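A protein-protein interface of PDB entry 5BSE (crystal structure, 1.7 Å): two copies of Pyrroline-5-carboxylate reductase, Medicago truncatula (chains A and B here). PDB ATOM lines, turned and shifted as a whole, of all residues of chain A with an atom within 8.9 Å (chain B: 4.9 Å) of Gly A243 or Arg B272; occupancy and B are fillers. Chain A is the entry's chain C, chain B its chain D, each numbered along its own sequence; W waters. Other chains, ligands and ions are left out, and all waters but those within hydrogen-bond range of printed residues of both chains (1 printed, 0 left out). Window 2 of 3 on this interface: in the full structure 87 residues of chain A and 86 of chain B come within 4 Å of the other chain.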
ATOM      1  N   VAL A 239     -24.057 -21.913  16.002  1.00  0.00           N
ATOM      2  CA  VAL A 239     -25.045 -21.620  14.954  1.00  0.00           C
ATOM      3  C   VAL A 239     -25.187 -20.149  14.624  1.00  0.00           C
ATOM      4  O   VAL A 239     -25.950 -19.793  13.752  1.00  0.00           O
ATOM      5  CB  VAL A 239     -26.460 -22.209  15.270  1.00  0.00           C
ATOM      6  CG1 VAL A 239     -26.370 -23.719  15.275  1.00  0.00           C
ATOM      7  CG2 VAL A 239     -26.966 -21.733  16.613  1.00  0.00           C
ATOM      8  N   THR A 240     -24.481 -19.261  15.324  1.00  0.00           N
ATOM      9  CA  THR A 240     -24.608 -17.857  15.066  1.00  0.00           C
ATOM     10  C   THR A 240     -23.505 -17.361  14.126  1.00  0.00           C
ATOM     11  O   THR A 240     -22.494 -16.781  14.527  1.00  0.00           O
ATOM     12  CB  THR A 240     -24.649 -17.049  16.369  1.00  0.00           C
ATOM     13  OG1 THR A 240     -23.669 -17.588  17.252  1.00  0.00           O
ATOM     14  CG2 THR A 240     -26.024 -17.187  17.031  1.00  0.00           C
ATOM     15  N   SER A 241     -23.688 -17.501  12.838  1.00  0.00           N
ATOM     16  CA  SER A 241     -22.680 -17.087  11.888  1.00  0.00           C
ATOM     17  C   SER A 241     -22.614 -15.531  11.887  1.00  0.00           C
ATOM     18  O   SER A 241     -23.593 -14.854  12.137  1.00  0.00           O
ATOM     19  CB  SER A 241     -22.989 -17.718  10.514  1.00  0.00           C
ATOM     20  OG  SER A 241     -24.083 -17.051  10.034  1.00  0.00           O
ATOM     21  N   PRO A 242     -21.484 -14.934  11.555  1.00  0.00           N
ATOM     22  CA  PRO A 242     -21.254 -13.473  11.624  1.00  0.00           C
ATOM     23  C   PRO A 242     -22.248 -12.731  10.780  1.00  0.00           C
ATOM     24  O   PRO A 242     -22.386 -12.980   9.587  1.00  0.00           O
ATOM     25  CB  PRO A 242     -19.841 -13.290  11.053  1.00  0.00           C
ATOM     26  CG  PRO A 242     -19.220 -14.599  11.383  1.00  0.00           C
ATOM     27  CD  PRO A 242     -20.230 -15.689  11.287  1.00  0.00           C
ATOM     28  N   GLY A 243     -22.920 -11.809  11.404  1.00  0.00           N
ATOM     29  CA  GLY A 243     -23.881 -10.961  10.805  1.00  0.00           C
ATOM     30  C   GLY A 243     -25.044 -11.711  10.106  1.00  0.00           C
ATOM     31  O   GLY A 243     -25.704 -11.153   9.220  1.00  0.00           O
ATOM     32  N   GLY A 244     -25.288 -12.936  10.489  1.00  0.00           N
ATOM     33  CA  GLY A 244     -26.242 -13.764   9.844  1.00  0.00           C
ATOM     34  C   GLY A 244     -27.668 -13.662  10.381  1.00  0.00           C
ATOM     35  O   GLY A 244     -27.975 -12.874  11.287  1.00  0.00           O
ATOM     36  N   THR A 245     -28.491 -14.574   9.884  1.00  0.00           N
ATOM     37  CA  THR A 245     -29.894 -14.568  10.271  1.00  0.00           C
ATOM     38  C   THR A 245     -30.070 -14.952  11.715  1.00  0.00           C
ATOM     39  O   THR A 245     -30.859 -14.392  12.405  1.00  0.00           O
ATOM     40  CB  THR A 245     -30.697 -15.520   9.372  1.00  0.00           C
ATOM     41  OG1 THR A 245     -30.243 -16.837   9.532  1.00  0.00           O
ATOM     42  CG2 THR A 245     -30.493 -15.127   7.937  1.00  0.00           C
ATOM     43  N   THR A 246     -29.321 -15.939  12.156  1.00  0.00           N
ATOM     44  CA  THR A 246     -29.488 -16.452  13.551  1.00  0.00           C
ATOM     45  C   THR A 246     -29.152 -15.417  14.568  1.00  0.00           C
ATOM     46  O   THR A 246     -29.873 -15.230  15.513  1.00  0.00           O
ATOM     47  CB  THR A 246     -28.696 -17.711  13.737  1.00  0.00           C
ATOM     48  OG1 THR A 246     -29.084 -18.617  12.671  1.00  0.00           O
ATOM     49  CG2 THR A 246     -28.953 -18.324  15.007  1.00  0.00           C
ATOM     50  N   ILE A 247     -27.989 -14.757  14.411  1.00  0.00           N
ATOM     51  CA  ILE A 247     -27.656 -13.746  15.382  1.00  0.00           C
ATOM     52  C   ILE A 247     -28.600 -12.563  15.370  1.00  0.00           C
ATOM     53  O   ILE A 247     -28.899 -11.962  16.368  1.00  0.00           O
ATOM     54  CB  ILE A 247     -26.192 -13.303  15.265  1.00  0.00           C
ATOM     55  CG1 ILE A 247     -25.721 -12.500  16.467  1.00  0.00           C
ATOM     56  CG2 ILE A 247     -25.981 -12.463  14.028  1.00  0.00           C
ATOM     57  CD1 ILE A 247     -25.598 -13.320  17.761  1.00  0.00           C
ATOM     58  N   ALA A 248     -29.196 -12.268  14.188  1.00  0.00           N
ATOM     59  CA  ALA A 248     -30.233 -11.246  14.159  1.00  0.00           C
ATOM     60  C   ALA A 248     -31.420 -11.659  15.046  1.00  0.00           C
ATOM     61  O   ALA A 248     -31.990 -10.843  15.756  1.00  0.00           O
ATOM     62  CB  ALA A 248     -30.701 -10.967  12.696  1.00  0.00           C
ATOM     63  N   GLY A 249     -31.832 -12.901  14.956  1.00  0.00           N
ATOM     64  CA  GLY A 249     -32.919 -13.381  15.789  1.00  0.00           C
ATOM     65  C   GLY A 249     -32.577 -13.419  17.259  1.00  0.00           C
ATOM     66  O   GLY A 249     -33.305 -12.971  18.121  1.00  0.00           O
ATOM     67  N   ALA B 268     -37.369 -11.039  12.512  1.00  0.00           N
ATOM     68  CA  ALA B 268     -36.120 -10.412  12.301  1.00  0.00           C
ATOM     69  C   ALA B 268     -35.131 -11.277  11.562  1.00  0.00           C
ATOM     70  O   ALA B 268     -34.425 -10.787  10.658  1.00  0.00           O
ATOM     71  CB  ALA B 268     -35.504  -9.969  13.589  1.00  0.00           C
ATOM     72  N   ALA B 269     -35.095 -12.553  11.937  1.00  0.00           N
ATOM     73  CA  ALA B 269     -34.202 -13.468  11.258  1.00  0.00           C
ATOM     74  C   ALA B 269     -34.606 -13.602   9.791  1.00  0.00           C
ATOM     75  O   ALA B 269     -33.760 -13.663   8.879  1.00  0.00           O
ATOM     76  CB  ALA B 269     -34.164 -14.798  11.945  1.00  0.00           C
ATOM     77  N   ALA B 270     -35.911 -13.701   9.554  1.00  0.00           N
ATOM     78  CA  ALA B 270     -36.386 -13.812   8.190  1.00  0.00           C
ATOM     79  C   ALA B 270     -36.091 -12.581   7.346  1.00  0.00           C
ATOM     80  O   ALA B 270     -35.708 -12.693   6.147  1.00  0.00           O
ATOM     81  CB  ALA B 270     -37.874 -14.123   8.155  1.00  0.00           C
ATOM     82  N   LYS B 271     -36.223 -11.418   7.935  1.00  0.00           N
ATOM     83  CA  LYS B 271     -35.906 -10.183   7.255  1.00  0.00           C
ATOM     84  C   LYS B 271     -34.398 -10.119   6.933  1.00  0.00           C
ATOM     85  O   LYS B 271     -33.995  -9.736   5.847  1.00  0.00           O
ATOM     86  CB  LYS B 271     -36.264  -9.039   8.115  1.00  0.00           C
ATOM     87  CG  LYS B 271     -35.839  -7.697   7.546  1.00  0.00           C
ATOM     88  CD  LYS B 271     -36.376  -6.524   8.351  1.00  0.00           C
ATOM     89  CE  LYS B 271     -35.894  -5.206   7.743  1.00  0.00           C
ATOM     90  NZ  LYS B 271     -35.988  -4.189   8.818  1.00  0.00           N
ATOM     91  N   ARG B 272     -33.575 -10.518   7.902  1.00  0.00           N
ATOM     92  CA  ARG B 272     -32.137 -10.598   7.640  1.00  0.00           C
ATOM     93  C   ARG B 272     -31.803 -11.553   6.506  1.00  0.00           C
ATOM     94  O   ARG B 272     -30.953 -11.281   5.638  1.00  0.00           O
ATOM     95  CB  ARG B 272     -31.416 -10.996   8.891  1.00  0.00           C
ATOM     96  CG  ARG B 272     -29.892 -10.949   8.701  1.00  0.00           C
ATOM     97  CD  ARG B 272     -29.397  -9.574   8.309  1.00  0.00           C
ATOM     98  NE  ARG B 272     -27.954  -9.495   8.322  1.00  0.00           N
ATOM     99  CZ  ARG B 272     -27.172  -8.740   7.564  1.00  0.00           C
ATOM    100  NH1 ARG B 272     -27.648  -7.983   6.590  1.00  0.00           N
ATOM    101  NH2 ARG B 272     -25.851  -8.802   7.785  1.00  0.00           N
ATOM    102  N   SER B 273     -32.471 -12.695   6.488  1.00  0.00           N
ATOM    103  CA  SER B 273     -32.297 -13.651   5.407  1.00  0.00           C
ATOM    104  C   SER B 273     -32.555 -12.996   4.053  1.00  0.00           C
ATOM    105  O   SER B 273     -31.815 -13.185   3.102  1.00  0.00           O
ATOM    106  CB  SER B 273     -33.245 -14.840   5.608  1.00  0.00           C
ATOM    107  OG  SER B 273     -33.045 -15.838   4.618  1.00  0.00           O
ATOM    108  N   GLN B 274     -33.673 -12.279   3.970  1.00  0.00           N
ATOM    109  CA  GLN B 274     -34.029 -11.600   2.722  1.00  0.00           C
ATOM    110  C   GLN B 274     -32.978 -10.560   2.362  1.00  0.00           C
ATOM    111  O   GLN B 274     -32.587 -10.422   1.180  1.00  0.00           O
ATOM    112  CB  GLN B 274     -35.411 -10.952   2.858  1.00  0.00           C
ATOM    113  CG  GLN B 274     -35.972 -10.462   1.545  1.00  0.00           C
ATOM    114  CD  GLN B 274     -35.338  -9.169   1.096  1.00  0.00           C
ATOM    115  OE1 GLN B 274     -35.044  -8.289   1.903  1.00  0.00           O
ATOM    116  NE2 GLN B 274     -35.115  -9.044  -0.231  1.00  0.00           N
ATOM    117  N   GLU B 275     -32.463  -9.824   3.346  1.00  0.00           N
ATOM    118  CA  GLU B 275     -31.481  -8.812   3.095  1.00  0.00           C
ATOM    119  C   GLU B 275     -30.198  -9.418   2.580  1.00  0.00           C
ATOM    120  O   GLU B 275     -29.476  -8.750   1.860  1.00  0.00           O
ATOM    121  CB  GLU B 275     -31.108  -8.052   4.339  1.00  0.00           C
ATOM    122  CG  GLU B 275     -32.179  -7.162   4.860  1.00  0.00           C
ATOM    123  CD  GLU B 275     -31.795  -6.571   6.206  1.00  0.00           C
ATOM    124  OE1 GLU B 275     -30.649  -6.846   6.778  1.00  0.00           O
ATOM    125  OE2 GLU B 275     -32.675  -5.813   6.666  1.00  0.00           O
ATOM    126  N   LEU B 276     -29.892 -10.637   2.991  1.00  0.00           N
ATOM    127  CA  LEU B 276     -28.605 -11.267   2.682  1.00  0.00           C
ATOM    128  C   LEU B 276     -28.696 -11.907   1.317  1.00  0.00           C
ATOM    129  O   LEU B 276     -27.740 -12.451   0.828  1.00  0.00           O
ATOM    130  CB  LEU B 276     -28.197 -12.327   3.709  1.00  0.00           C
ATOM    131  CG  LEU B 276     -27.727 -11.702   5.013  1.00  0.00           C
ATOM    132  CD1 LEU B 276     -27.604 -12.798   6.023  1.00  0.00           C
ATOM    133  CD2 LEU B 276     -26.403 -10.915   4.843  1.00  0.00           C
HETATM  134  O   HOH W   1     -27.473 -10.197  11.361  1.00  0.00           O
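Val A239 touches none of the printed residues of chain B.
Of the printed residues of chain B, Gly A243 touches Arg B272 (2.8 Å).
Printed residues of chain B within 4 Å of Gly A244: Arg B272.
Of the printed residues of chain B, Thr A245 touches Ala B269 (3.4 Å), Arg B272 (3.9 Å) and Ser B273 (3.4 Å).
Printed residues of chain B within 4 Å of Ala A248: Arg B272.
Of the printed residues of chain A, Ala B269 touches Thr A245.
Printed residues of chain A within 4 Å of Arg B272: Gly A243, Gly A244, Thr A245 and Ala A248.
Of chain A, only Thr A245 (3.4 Å) comes within 4 Å of Ser B273.
The backbone carbonyl oxygen of Gly A243 lies within hydrogen-bond range of the guanidinium group of Arg B272, 2.8 Å away.
Of the 9 printed residues of chain B, 3 touch a printed residue of chain A.
Along chain B the printed residues that touch a printed residue of chain A span positions 269 to 273.
Hydrophobic or aromatic side chains of chain A that line the printed part of chain B: Ala A248.
Among the printed residues, 6 pairs touch across the chains.
No position is printed for both chains.
Of the 6 pairs that touch across the chains among the printed residues, none has its exchanged pair printed and touching as well.
OE1 of Glu B275 is in salt-bridge range of NH1 of Arg B272, at 3.2 Å.
Among the printed residues, pairs that only touch across the chains: Thr A245 with Ala B269 (3.4 Å), Thr A245 with Ser B273 (3.4 Å), Gly A244 with Arg B272 (3.8 Å), Ala A248 with Arg B272 (3.9 Å) and Thr A245 with Arg B272 (3.9 Å).
Water W1 lies within hydrogen-bond range of O of Gly A244 (2.7 Å), O of Gly A243 (2.9 Å) and NE of Arg B272 (3.2 Å).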
